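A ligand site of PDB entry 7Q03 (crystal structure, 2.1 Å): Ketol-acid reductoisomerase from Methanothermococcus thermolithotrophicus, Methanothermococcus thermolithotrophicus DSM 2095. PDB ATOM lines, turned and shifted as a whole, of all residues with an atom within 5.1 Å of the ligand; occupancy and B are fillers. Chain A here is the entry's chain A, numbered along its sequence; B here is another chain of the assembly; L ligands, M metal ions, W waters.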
ATOM      1  N   GLY A  24     -13.719 -12.312  27.166  1.00  0.00           N
ATOM      2  CA  GLY A  24     -13.555 -10.936  26.745  1.00  0.00           C
ATOM      3  C   GLY A  24     -13.838 -10.696  25.265  1.00  0.00           C
ATOM      4  O   GLY A  24     -13.686 -11.597  24.430  1.00  0.00           O
ATOM      5  N   TYR A  25     -14.259  -9.478  24.935  1.00  0.00           N
ATOM      6  CA  TYR A  25     -14.588  -9.123  23.550  1.00  0.00           C
ATOM      7  C   TYR A  25     -14.269  -7.654  23.303  1.00  0.00           C
ATOM      8  O   TYR A  25     -15.021  -6.938  22.631  1.00  0.00           O
ATOM      9  CB  TYR A  25     -16.058  -9.416  23.231  1.00  0.00           C
ATOM     10  CG  TYR A  25     -16.307  -9.862  21.817  1.00  0.00           C
ATOM     11  CD1 TYR A  25     -15.791 -11.075  21.350  1.00  0.00           C
ATOM     12  CD2 TYR A  25     -17.051  -9.092  20.943  1.00  0.00           C
ATOM     13  CE1 TYR A  25     -16.020 -11.490  20.049  1.00  0.00           C
ATOM     14  CE2 TYR A  25     -17.288  -9.495  19.641  1.00  0.00           C
ATOM     15  CZ  TYR A  25     -16.763 -10.699  19.204  1.00  0.00           C
ATOM     16  OH  TYR A  25     -16.994 -11.106  17.914  1.00  0.00           O
ATOM     17  N   GLY A  26     -13.154  -7.186  23.858  1.00  0.00           N
ATOM     18  CA  GLY A  26     -12.735  -5.815  23.656  1.00  0.00           C
ATOM     19  C   GLY A  26     -11.862  -5.646  22.434  1.00  0.00           C
ATOM     20  O   GLY A  26     -12.149  -6.220  21.381  1.00  0.00           O
ATOM     21  N   SER A  27     -10.790  -4.861  22.559  1.00  0.00           N
ATOM     22  CA  SER A  27      -9.858  -4.676  21.442  1.00  0.00           C
ATOM     23  C   SER A  27      -9.292  -6.011  20.973  1.00  0.00           C
ATOM     24  O   SER A  27      -9.537  -6.443  19.838  1.00  0.00           O
ATOM     25  CB  SER A  27      -8.745  -3.724  21.851  1.00  0.00           C
ATOM     26  OG  SER A  27      -7.948  -3.383  20.739  1.00  0.00           O
ATOM     27  N   GLN A  28      -8.530  -6.688  21.838  1.00  0.00           N
ATOM     28  CA  GLN A  28      -7.986  -7.988  21.472  1.00  0.00           C
ATOM     29  C   GLN A  28      -9.046  -9.080  21.520  1.00  0.00           C
ATOM     30  O   GLN A  28      -9.087  -9.935  20.624  1.00  0.00           O
ATOM     31  CB  GLN A  28      -6.834  -8.341  22.406  1.00  0.00           C
ATOM     32  CG  GLN A  28      -5.630  -7.433  22.244  1.00  0.00           C
ATOM     33  CD  GLN A  28      -4.819  -7.737  20.999  1.00  0.00           C
ATOM     34  OE1 GLN A  28      -4.953  -8.792  20.399  1.00  0.00           O
ATOM     35  NE2 GLN A  28      -3.981  -6.792  20.600  1.00  0.00           N
ATOM     36  N   GLY A  29      -9.889  -9.081  22.544  1.00  0.00           N
ATOM     37  CA  GLY A  29     -10.941 -10.069  22.722  1.00  0.00           C
ATOM     38  C   GLY A  29     -11.730 -10.351  21.472  1.00  0.00           C
ATOM     39  O   GLY A  29     -11.736 -11.480  20.966  1.00  0.00           O
ATOM     40  N   LEU A  47     -18.808 -13.672  28.308  1.00  0.00           N
ATOM     41  CA  LEU A  47     -19.032 -12.227  28.600  1.00  0.00           C
ATOM     42  C   LEU A  47     -20.002 -12.021  29.769  1.00  0.00           C
ATOM     43  O   LEU A  47     -20.654 -12.967  30.171  1.00  0.00           O
ATOM     44  CB  LEU A  47     -19.690 -11.604  27.374  1.00  0.00           C
ATOM     45  CG  LEU A  47     -18.818 -11.365  26.147  1.00  0.00           C
ATOM     46  CD1 LEU A  47     -17.347 -11.352  26.504  1.00  0.00           C
ATOM     47  CD2 LEU A  47     -19.105 -12.399  25.083  1.00  0.00           C
ATOM     48  N   ARG A  48     -20.093 -10.772  30.242  1.00  0.00           N
ATOM     49  CA  ARG A  48     -21.050 -10.413  31.315  1.00  0.00           C
ATOM     50  C   ARG A  48     -22.462 -10.345  30.722  1.00  0.00           C
ATOM     51  O   ARG A  48     -22.598  -9.810  29.597  1.00  0.00           O
ATOM     52  CB  ARG A  48     -20.688  -9.046  31.908  1.00  0.00           C
ATOM     53  CG  ARG A  48     -19.243  -8.905  32.363  1.00  0.00           C
ATOM     54  CD  ARG A  48     -19.090  -7.797  33.384  1.00  0.00           C
ATOM     55  NE  ARG A  48     -18.792  -6.512  32.755  1.00  0.00           N
ATOM     56  CZ  ARG A  48     -18.441  -5.422  33.426  1.00  0.00           C
ATOM     57  NH1 ARG A  48     -18.338  -5.446  34.738  1.00  0.00           N
ATOM     58  NH2 ARG A  48     -18.190  -4.300  32.762  1.00  0.00           N
ATOM     59  N   GLY A  51     -23.581  -6.731  30.602  1.00  0.00           N
ATOM     60  CA  GLY A  51     -22.591  -5.917  29.870  1.00  0.00           C
ATOM     61  C   GLY A  51     -22.950  -5.662  28.416  1.00  0.00           C
ATOM     62  O   GLY A  51     -23.718  -6.436  27.855  1.00  0.00           O
ATOM     63  N   ALA A  52     -22.296  -4.666  27.806  1.00  0.00           N
ATOM     64  CA  ALA A  52     -22.535  -4.264  26.396  1.00  0.00           C
ATOM     65  C   ALA A  52     -21.957  -5.274  25.397  1.00  0.00           C
ATOM     66  O   ALA A  52     -22.730  -5.737  24.531  1.00  0.00           O
ATOM     67  CB  ALA A  52     -21.992  -2.874  26.161  1.00  0.00           C
ATOM     68  N   SER A  53     -20.660  -5.596  25.500  1.00  0.00           N
ATOM     69  CA  SER A  53     -20.024  -6.525  24.526  1.00  0.00           C
ATOM     70  C   SER A  53     -20.829  -7.829  24.379  1.00  0.00           C
ATOM     71  O   SER A  53     -20.729  -8.433  23.292  1.00  0.00           O
ATOM     72  CB  SER A  53     -18.573  -6.807  24.814  1.00  0.00           C
ATOM     73  OG  SER A  53     -18.415  -7.421  26.085  1.00  0.00           O
ATOM     74  N   TRP A  54     -21.543  -8.263  25.424  1.00  0.00           N
ATOM     75  CA  TRP A  54     -22.336  -9.516  25.244  1.00  0.00           C
ATOM     76  C   TRP A  54     -23.265  -9.449  24.029  1.00  0.00           C
ATOM     77  O   TRP A  54     -23.291 -10.425  23.273  1.00  0.00           O
ATOM     78  CB  TRP A  54     -23.127  -9.769  26.532  1.00  0.00           C
ATOM     79  CG  TRP A  54     -24.476 -10.408  26.408  1.00  0.00           C
ATOM     80  CD1 TRP A  54     -24.736 -11.708  26.059  1.00  0.00           C
ATOM     81  CD2 TRP A  54     -25.750  -9.811  26.712  1.00  0.00           C
ATOM     82  NE1 TRP A  54     -26.082 -11.943  26.108  1.00  0.00           N
ATOM     83  CE2 TRP A  54     -26.731 -10.799  26.502  1.00  0.00           C
ATOM     84  CE3 TRP A  54     -26.163  -8.536  27.086  1.00  0.00           C
ATOM     85  CZ2 TRP A  54     -28.093 -10.550  26.683  1.00  0.00           C
ATOM     86  CZ3 TRP A  54     -27.498  -8.300  27.298  1.00  0.00           C
ATOM     87  CH2 TRP A  54     -28.449  -9.285  27.075  1.00  0.00           C
ATOM     88  N   ILE A  67     -19.234 -16.297  31.610  1.00  0.00           N
ATOM     89  CA  ILE A  67     -17.818 -16.575  31.818  1.00  0.00           C
ATOM     90  C   ILE A  67     -17.655 -17.906  32.543  1.00  0.00           C
ATOM     91  O   ILE A  67     -16.853 -18.760  32.133  1.00  0.00           O
ATOM     92  CB  ILE A  67     -17.158 -15.431  32.616  1.00  0.00           C
ATOM     93  CG1 ILE A  67     -17.234 -14.118  31.843  1.00  0.00           C
ATOM     94  CG2 ILE A  67     -15.718 -15.780  32.948  1.00  0.00           C
ATOM     95  CD1 ILE A  67     -16.859 -12.893  32.668  1.00  0.00           C
ATOM     96  N   ILE A  79      -7.783 -15.308  28.285  1.00  0.00           N
ATOM     97  CA  ILE A  79      -8.253 -14.170  29.076  1.00  0.00           C
ATOM     98  C   ILE A  79      -7.886 -12.893  28.344  1.00  0.00           C
ATOM     99  O   ILE A  79      -6.707 -12.552  28.197  1.00  0.00           O
ATOM    100  CB  ILE A  79      -7.653 -14.195  30.494  1.00  0.00           C
ATOM    101  CG1 ILE A  79      -7.963 -15.538  31.161  1.00  0.00           C
ATOM    102  CG2 ILE A  79      -8.180 -13.035  31.319  1.00  0.00           C
ATOM    103  CD1 ILE A  79      -7.714 -15.565  32.651  1.00  0.00           C
ATOM    104  N   LEU A  80      -8.920 -12.207  27.856  1.00  0.00           N
ATOM    105  CA  LEU A  80      -8.725 -10.977  27.053  1.00  0.00           C
ATOM    106  C   LEU A  80      -9.565  -9.840  27.624  1.00  0.00           C
ATOM    107  O   LEU A  80     -10.419  -9.326  26.933  1.00  0.00           O
ATOM    108  CB  LEU A  80      -9.057 -11.293  25.603  1.00  0.00           C
ATOM    109  CG  LEU A  80      -8.065 -12.243  24.940  1.00  0.00           C
ATOM    110  CD1 LEU A  80      -8.380 -12.459  23.475  1.00  0.00           C
ATOM    111  CD2 LEU A  80      -6.648 -11.728  25.093  1.00  0.00           C
ATOM    112  N   ILE A  81      -9.326  -9.527  28.884  1.00  0.00           N
ATOM    113  CA  ILE A  81      -9.953  -8.355  29.560  1.00  0.00           C
ATOM    114  C   ILE A  81      -8.822  -7.446  30.063  1.00  0.00           C
ATOM    115  O   ILE A  81      -7.665  -7.864  30.039  1.00  0.00           O
ATOM    116  CB  ILE A  81     -10.950  -8.795  30.650  1.00  0.00           C
ATOM    117  CG1 ILE A  81     -10.255  -9.364  31.881  1.00  0.00           C
ATOM    118  CG2 ILE A  81     -11.958  -9.767  30.083  1.00  0.00           C
ATOM    119  CD1 ILE A  81     -11.204  -9.913  32.916  1.00  0.00           C
ATOM    120  N   PRO A  82      -9.081  -6.218  30.518  1.00  0.00           N
ATOM    121  CA  PRO A  82      -8.018  -5.329  30.944  1.00  0.00           C
ATOM    122  C   PRO A  82      -7.280  -5.938  32.151  1.00  0.00           C
ATOM    123  O   PRO A  82      -7.914  -6.503  33.005  1.00  0.00           O
ATOM    124  CB  PRO A  82      -8.736  -4.034  31.333  1.00  0.00           C
ATOM    125  CG  PRO A  82     -10.080  -4.131  30.692  1.00  0.00           C
ATOM    126  CD  PRO A  82     -10.401  -5.606  30.637  1.00  0.00           C
ATOM    127  N   ASP A  83      -5.962  -5.756  32.150  1.00  0.00           N
ATOM    128  CA  ASP A  83      -5.059  -6.325  33.177  1.00  0.00           C
ATOM    129  C   ASP A  83      -5.461  -5.888  34.584  1.00  0.00           C
ATOM    130  O   ASP A  83      -5.451  -6.748  35.465  1.00  0.00           O
ATOM    131  CB  ASP A  83      -3.614  -5.935  32.891  1.00  0.00           C
ATOM    132  CG  ASP A  83      -3.187  -6.204  31.459  1.00  0.00           C
ATOM    133  OD1 ASP A  83      -3.007  -7.367  31.119  1.00  0.00           O
ATOM    134  OD2 ASP A  83      -3.037  -5.242  30.713  1.00  0.00           O
ATOM    135  N   ILE A  85      -8.133  -5.471  36.006  1.00  0.00           N
ATOM    136  CA  ILE A  85      -9.320  -6.149  36.614  1.00  0.00           C
ATOM    137  C   ILE A  85      -9.267  -7.665  36.390  1.00  0.00           C
ATOM    138  O   ILE A  85     -10.256  -8.337  36.752  1.00  0.00           O
ATOM    139  CB  ILE A  85     -10.632  -5.543  36.066  1.00  0.00           C
ATOM    140  CG1 ILE A  85     -10.717  -5.644  34.540  1.00  0.00           C
ATOM    141  CG2 ILE A  85     -10.796  -4.101  36.539  1.00  0.00           C
ATOM    142  CD1 ILE A  85     -11.600  -6.766  34.049  1.00  0.00           C
ATOM    143  N   GLN A  86      -8.173  -8.187  35.823  1.00  0.00           N
ATOM    144  CA  GLN A  86      -8.073  -9.623  35.605  1.00  0.00           C
ATOM    145  C   GLN A  86      -7.956 -10.399  36.911  1.00  0.00           C
ATOM    146  O   GLN A  86      -8.428 -11.534  36.999  1.00  0.00           O
ATOM    147  CB  GLN A  86      -6.882  -9.953  34.714  1.00  0.00           C
ATOM    148  CG  GLN A  86      -7.114  -9.719  33.240  1.00  0.00           C
ATOM    149  CD  GLN A  86      -5.989 -10.230  32.375  1.00  0.00           C
ATOM    150  OE1 GLN A  86      -5.114 -10.956  32.852  1.00  0.00           O
ATOM    151  NE2 GLN A  86      -5.998  -9.848  31.112  1.00  0.00           N
ATOM    152  N   VAL A  89     -11.580 -10.949  38.359  1.00  0.00           N
ATOM    153  CA  VAL A  89     -12.399 -11.817  37.512  1.00  0.00           C
ATOM    154  C   VAL A  89     -11.884 -13.251  37.565  1.00  0.00           C
ATOM    155  O   VAL A  89     -12.672 -14.216  37.534  1.00  0.00           O
ATOM    156  CB  VAL A  89     -12.437 -11.267  36.073  1.00  0.00           C
ATOM    157  CG1 VAL A  89     -13.131 -12.252  35.140  1.00  0.00           C
ATOM    158  CG2 VAL A  89     -13.131  -9.913  36.041  1.00  0.00           C
ATOM    159  N   GLN A  93     -14.580 -15.893  38.907  1.00  0.00           N
ATOM    160  CA  GLN A  93     -15.338 -16.520  37.826  1.00  0.00           C
ATOM    161  C   GLN A  93     -14.505 -17.436  36.943  1.00  0.00           C
ATOM    162  O   GLN A  93     -14.938 -17.760  35.835  1.00  0.00           O
ATOM    163  CB  GLN A  93     -16.010 -15.457  36.945  1.00  0.00           C
ATOM    164  CG  GLN A  93     -16.714 -14.340  37.670  1.00  0.00           C
ATOM    165  CD  GLN A  93     -17.322 -13.332  36.725  1.00  0.00           C
ATOM    166  OE1 GLN A  93     -16.645 -12.416  36.262  1.00  0.00           O
ATOM    167  NE2 GLN A  93     -18.600 -13.498  36.417  1.00  0.00           N
ATOM    168  N   SER A 107      -2.481 -13.010  26.635  1.00  0.00           N
ATOM    169  CA  SER A 107      -1.782 -12.315  25.562  1.00  0.00           C
ATOM    170  C   SER A 107      -0.816 -11.269  26.096  1.00  0.00           C
ATOM    171  O   SER A 107      -0.235 -10.510  25.313  1.00  0.00           O
ATOM    172  CB  SER A 107      -2.788 -11.668  24.600  1.00  0.00           C
ATOM    173  OG  SER A 107      -3.138 -12.569  23.572  1.00  0.00           O
ATOM    174  N   HIS A 108      -0.622 -11.217  27.406  1.00  0.00           N
ATOM    175  CA  HIS A 108       0.298 -10.287  28.038  1.00  0.00           C
ATOM    176  C   HIS A 108       0.686 -10.865  29.399  1.00  0.00           C
ATOM    177  O   HIS A 108      -0.182 -11.339  30.136  1.00  0.00           O
ATOM    178  CB  HIS A 108      -0.313  -8.893  28.195  1.00  0.00           C
ATOM    179  CG  HIS A 108       0.651  -7.869  28.717  1.00  0.00           C
ATOM    180  ND1 HIS A 108       1.984  -7.842  28.356  1.00  0.00           N
ATOM    181  CD2 HIS A 108       0.467  -6.823  29.549  1.00  0.00           C
ATOM    182  CE1 HIS A 108       2.574  -6.826  28.959  1.00  0.00           C
ATOM    183  NE2 HIS A 108       1.685  -6.192  29.688  1.00  0.00           N
ATOM    184  N   PRO A 130       0.019 -11.102  20.520  1.00  0.00           N
ATOM    185  CA  PRO A 130       0.248 -10.346  19.286  1.00  0.00           C
ATOM    186  C   PRO A 130       0.895  -8.983  19.562  1.00  0.00           C
ATOM    187  O   PRO A 130       0.514  -8.274  20.486  1.00  0.00           O
ATOM    188  CB  PRO A 130      -1.167 -10.164  18.716  1.00  0.00           C
ATOM    189  CG  PRO A 130      -2.065 -11.089  19.510  1.00  0.00           C
ATOM    190  CD  PRO A 130      -1.410 -11.202  20.852  1.00  0.00           C
ATOM    191  N   SER A 132       0.700  -6.008  18.270  1.00  0.00           N
ATOM    192  CA  SER A 132      -0.030  -4.973  17.492  1.00  0.00           C
ATOM    193  C   SER A 132      -1.347  -4.626  18.207  1.00  0.00           C
ATOM    194  O   SER A 132      -1.815  -5.442  19.007  1.00  0.00           O
ATOM    195  CB  SER A 132      -0.285  -5.416  16.066  1.00  0.00           C
ATOM    196  OG  SER A 132      -1.646  -5.744  15.846  1.00  0.00           O
ATOM    197  N   PRO A 133      -1.955  -3.455  17.926  1.00  0.00           N
ATOM    198  CA  PRO A 133      -3.246  -3.106  18.522  1.00  0.00           C
ATOM    199  C   PRO A 133      -4.316  -4.102  18.030  1.00  0.00           C
ATOM    200  O   PRO A 133      -4.271  -4.503  16.886  1.00  0.00           O
ATOM    201  CB  PRO A 133      -3.523  -1.677  18.012  1.00  0.00           C
ATOM    202  CG  PRO A 133      -2.633  -1.531  16.792  1.00  0.00           C
ATOM    203  CD  PRO A 133      -1.431  -2.399  17.064  1.00  0.00           C
ATOM    204  N   GLY A 134      -5.259  -4.437  18.900  1.00  0.00           N
ATOM    205  CA  GLY A 134      -6.290  -5.437  18.574  1.00  0.00           C
ATOM    206  C   GLY A 134      -7.014  -5.143  17.268  1.00  0.00           C
ATOM    207  O   GLY A 134      -7.273  -6.115  16.533  1.00  0.00           O
ATOM    208  N   ASP A 191       7.364  -5.030  26.267  1.00  0.00           N
ATOM    209  CA  ASP A 191       6.089  -4.468  25.827  1.00  0.00           C
ATOM    210  C   ASP A 191       5.793  -3.145  26.522  1.00  0.00           C
ATOM    211  O   ASP A 191       5.448  -2.157  25.879  1.00  0.00           O
ATOM    212  CB  ASP A 191       4.958  -5.474  26.089  1.00  0.00           C
ATOM    213  CG  ASP A 191       3.616  -4.973  25.618  1.00  0.00           C
ATOM    214  OD1 ASP A 191       3.320  -5.104  24.411  1.00  0.00           O
ATOM    215  OD2 ASP A 191       2.851  -4.460  26.463  1.00  0.00           O
ATOM    216  N   ASP B 250      -8.234   2.325  21.259  1.00  0.00           N
ATOM    217  CA  ASP B 250      -7.914   0.961  20.850  1.00  0.00           C
ATOM    218  C   ASP B 250      -6.802   0.368  21.708  1.00  0.00           C
ATOM    219  O   ASP B 250      -6.824  -0.839  22.013  1.00  0.00           O
ATOM    220  CB  ASP B 250      -7.533   0.921  19.381  1.00  0.00           C
ATOM    221  CG  ASP B 250      -7.604  -0.484  18.801  1.00  0.00           C
ATOM    222  OD1 ASP B 250      -8.677  -1.121  18.905  1.00  0.00           O
ATOM    223  OD2 ASP B 250      -6.582  -0.970  18.257  1.00  0.00           O
ATOM    224  N   VAL B 251      -5.811   1.173  22.091  1.00  0.00           N
ATOM    225  CA  VAL B 251      -4.743   0.645  22.939  1.00  0.00           C
ATOM    226  C   VAL B 251      -5.269   0.404  24.348  1.00  0.00           C
ATOM    227  O   VAL B 251      -6.253   1.008  24.800  1.00  0.00           O
ATOM    228  CB  VAL B 251      -3.519   1.580  22.953  1.00  0.00           C
ATOM    229  CG1 VAL B 251      -3.058   1.895  21.531  1.00  0.00           C
ATOM    230  CG2 VAL B 251      -3.799   2.852  23.749  1.00  0.00           C
ATOM    231  N   SER B 252      -4.591  -0.490  25.052  1.00  0.00           N
ATOM    232  CA  SER B 252      -4.992  -0.835  26.410  1.00  0.00           C
ATOM    233  C   SER B 252      -4.847   0.358  27.344  1.00  0.00           C
ATOM    234  O   SER B 252      -4.067   1.296  27.095  1.00  0.00           O
ATOM    235  CB  SER B 252      -4.158  -2.006  26.919  1.00  0.00           C
ATOM    236  OG  SER B 252      -2.822  -1.624  27.183  1.00  0.00           O
ATOM    237  N   ASN B 253      -5.594   0.327  28.442  1.00  0.00           N
ATOM    238  CA  ASN B 253      -5.446   1.361  29.461  1.00  0.00           C
ATOM    239  C   ASN B 253      -4.050   1.353  30.071  1.00  0.00           C
ATOM    240  O   ASN B 253      -3.544   2.399  30.497  1.00  0.00           O
ATOM    241  CB  ASN B 253      -6.495   1.174  30.548  1.00  0.00           C
ATOM    242  CG  ASN B 253      -7.878   0.859  29.982  1.00  0.00           C
ATOM    243  OD1 ASN B 253      -8.280   1.423  28.969  1.00  0.00           O
ATOM    244  ND2 ASN B 253      -8.591  -0.053  30.645  1.00  0.00           N
HETATM  245  P1  LIG L   1     -10.322  -4.247  26.884  1.00  0.00           P
HETATM  246  O1  LIG L   1     -10.727  -3.823  25.532  1.00  0.00           O
HETATM  247  O2  LIG L   1      -9.845  -3.063  27.679  1.00  0.00           O
HETATM  248  O3  LIG L   1     -11.490  -4.951  27.679  1.00  0.00           O
HETATM  249  C1  LIG L   1     -12.848  -4.814  27.232  1.00  0.00           C
HETATM  250  C2  LIG L   1     -13.582  -6.083  27.563  1.00  0.00           C
HETATM  251  O4  LIG L   1     -13.419  -6.384  28.966  1.00  0.00           O
HETATM  252  C3  LIG L   1     -15.090  -6.055  27.301  1.00  0.00           C
HETATM  253  O5  LIG L   1     -15.539  -7.288  26.764  1.00  0.00           O
HETATM  254  C4  LIG L   1     -15.654  -5.865  28.700  1.00  0.00           C
HETATM  255  O6  LIG L   1     -16.991  -6.398  28.811  1.00  0.00           O
HETATM  256  C5  LIG L   1     -14.688  -6.694  29.511  1.00  0.00           C
HETATM  257  N1  LIG L   1     -14.687  -6.389  30.931  1.00  0.00           N
HETATM  258  C6  LIG L   1     -14.287  -5.224  31.532  1.00  0.00           C
HETATM  259  N2  LIG L   1     -14.438  -5.217  32.834  1.00  0.00           N
HETATM  260  C7  LIG L   1     -14.966  -6.470  33.107  1.00  0.00           C
HETATM  261  C8  LIG L   1     -15.344  -7.092  34.314  1.00  0.00           C
HETATM  262  N3  LIG L   1     -15.275  -6.504  35.506  1.00  0.00           N
HETATM  263  N4  LIG L   1     -15.819  -8.356  34.238  1.00  0.00           N
HETATM  264  C9  LIG L   1     -15.902  -8.937  33.038  1.00  0.00           C
HETATM  265  N5  LIG L   1     -15.581  -8.445  31.841  1.00  0.00           N
HETATM  266  C10 LIG L   1     -15.122  -7.200  31.944  1.00  0.00           C
HETATM  267  O7  LIG L   1      -9.143  -5.307  26.798  1.00  0.00           O
HETATM  268  P2  LIG L   1      -7.858  -5.429  25.867  1.00  0.00           P
HETATM  269  O8  LIG L   1      -8.246  -5.929  24.543  1.00  0.00           O
HETATM  270  O9  LIG L   1      -7.261  -4.052  25.748  1.00  0.00           O
HETATM  271  O10 LIG L   1      -6.833  -6.312  26.666  1.00  0.00           O
HETATM  272  C11 LIG L   1      -6.749  -7.742  26.580  1.00  0.00           C
HETATM  273  C12 LIG L   1      -5.360  -8.216  26.929  1.00  0.00           C
HETATM  274  O11 LIG L   1      -4.517  -8.145  25.761  1.00  0.00           O
HETATM  275  C13 LIG L   1      -4.645  -7.426  28.019  1.00  0.00           C
HETATM  276  O12 LIG L   1      -3.931  -8.298  28.889  1.00  0.00           O
HETATM  277  C14 LIG L   1      -3.694  -6.530  27.231  1.00  0.00           C
HETATM  278  O13 LIG L   1      -2.539  -6.230  27.998  1.00  0.00           O
HETATM  279  C15 LIG L   1      -3.340  -7.429  26.058  1.00  0.00           C
HETATM  280  N6  LIG L   1      -2.901  -6.725  24.858  1.00  0.00           N
HETATM  281  C16 LIG L   1      -3.633  -5.681  24.354  1.00  0.00           C
HETATM  282  C17 LIG L   1      -3.272  -5.011  23.250  1.00  0.00           C
HETATM  283  C18 LIG L   1      -4.186  -3.981  22.720  1.00  0.00           C
HETATM  284  O14 LIG L   1      -3.999  -3.513  21.601  1.00  0.00           O
HETATM  285  N7  LIG L   1      -5.204  -3.610  23.485  1.00  0.00           N
HETATM  286  C19 LIG L   1      -2.000  -5.322  22.520  1.00  0.00           C
HETATM  287  C20 LIG L   1      -1.357  -6.525  23.100  1.00  0.00           C
HETATM  288  C21 LIG L   1      -1.794  -7.138  24.184  1.00  0.00           C
HETATM  289  P3  LIG L   1     -18.277  -5.507  28.889  1.00  0.00           P
HETATM  290  O15 LIG L   1     -18.752  -5.179  27.564  1.00  0.00           O
HETATM  291  O16 LIG L   1     -17.906  -4.324  29.673  1.00  0.00           O
HETATM  292  O17 LIG L   1     -19.270  -6.293  29.680  1.00  0.00           O
HETATM  293 MG    MG M   1       2.476  -4.198  22.400  1.00  0.00          MG
HETATM  294 MG    MG M   2       0.811  -3.625  26.094  1.00  0.00          MG
HETATM  295  O   HOH W   1       1.571  -6.738  22.974  1.00  0.00           O
HETATM  296  O   HOH W   2      -4.180 -11.331  28.808  1.00  0.00           O
HETATM  297  O   HOH W   3       0.120  -5.748  26.671  1.00  0.00           O
HETATM  298  O   HOH W   4      -8.694  -1.686  24.334  1.00  0.00           O
HETATM  299  O   HOH W   5     -10.561  -7.490  25.118  1.00  0.00           O
HETATM  300  O   HOH W   6      -7.500  -2.337  28.487  1.00  0.00           O
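The backbone NH (N) of Ser 27 sits at hydrogen-bond distance from an oxygen (O1) of the ligand. An oxygen (O12) of the ligand is in hydrogen-bond range of the side-chain amide nitrogen of Gln 86. N of Gln 28 is in hydrogen-bond range of O8 of the ligand (2.8 Å). The side-chain hydroxyl of Ser 53 is in hydrogen-bond range of an oxygen (O15) of the ligand (2.7 Å). The backbone NH (N) of Tyr 25 sits at hydrogen-bond distance from an oxygen (O5) of the ligand (3.1 Å). OD1 of Asp 83 sits at hydrogen-bond distance from O12 of the ligand (2.6 Å). An oxygen (O16) of the ligand is in salt-bridge range of the guanidinium group (NH2) of Arg 48, at 3.1 Å. N of Gly 134 lies within hydrogen-bond range of O14 of the ligand. The backbone NH of Ser 53 is in hydrogen-bond range of an oxygen (O15) of the ligand (2.8 Å). An oxygen (O14) of the ligand lies close to the side-chain amide nitrogen (NE2) of Gln 28 (3.4 Å).
N of Gly 134 sits close to OG of Ser 27 (3.4 Å). The side-chain amide nitrogen (NE2) of Gln 86 lies within hydrogen-bond range of the backbone carbonyl oxygen (O) of Ile 81 (2.8 Å). The side-chain amide nitrogen (NE2) of Gln 28 is in hydrogen-bond range of the backbone carbonyl oxygen (O) of Ser 132. The backbone NH (N) of Gly 134 sits close to the side-chain amide nitrogen (NE2) of Gln 28, at 3.2 Å. The side-chain hydroxyl of Ser 27 sits at hydrogen-bond distance from the side-chain carboxylate of Asp 250 of chain B, at 3.0 Å.
CA of Gly 26 touches O1 of the ligand, 3.4 Å away. Gly 51 touches the ligand. Ala 52 touches the ligand (N to O15, 3.6 Å). C of Leu 80 touches C11 of the ligand, 3.7 Å away. Ile 81 touches the ligand. CG of Pro 82 touches O2 of the ligand, 3.2 Å away. Ile 85 touches the ligand (CD1 to N2, 3.5 Å). Val 89 touches the ligand. O of Ser 107 touches C21 of the ligand, at 3.9 Å. His 108 touches the ligand (CD2 to O13, 3.4 Å). Pro 130 touches the ligand (O to C20, 3.7 Å). Ser 132 touches the ligand. Pro 133 touches the ligand. O of Asp 250 of chain B touches N7 of the ligand (3.5 Å). Ser 252 of chain B touches the ligand (N to N7, 3.5 Å). Of the 33 residues printed, 23 come within 4 Å of the ligand. Along chain A the residues within 4 Å of the ligand span positions 25 to 134. The nearest printed residue that does not touch the ligand is Gly 29 (4.1 Å).
Water W6 lies within hydrogen-bond range of an oxygen (O2) of the ligand (2.6 Å) and the backbone NH of Asn 253 of chain B (3.3 Å). Water W5 lies within hydrogen-bond range of O of Leu 80 (2.6 Å), O8 of the ligand (2.9 Å), N of Gly 26 (2.9 Å) and N of Gly 29 (3.1 Å). Water W3 bridges an oxygen (O13) of the ligand and a ring nitrogen (ND1) of His 108. Water W2 lies within hydrogen-bond range of O of Ile 79 (2.9 Å), O12 of the ligand (3.0 Å), N of Ser 107 (3.2 Å) and NE2 of Gln 86 (3.3 Å). Water W4 lies within hydrogen-bond range of O of Asp 250 of chain B (3.1 Å) and O9 of the ligand (3.1 Å).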
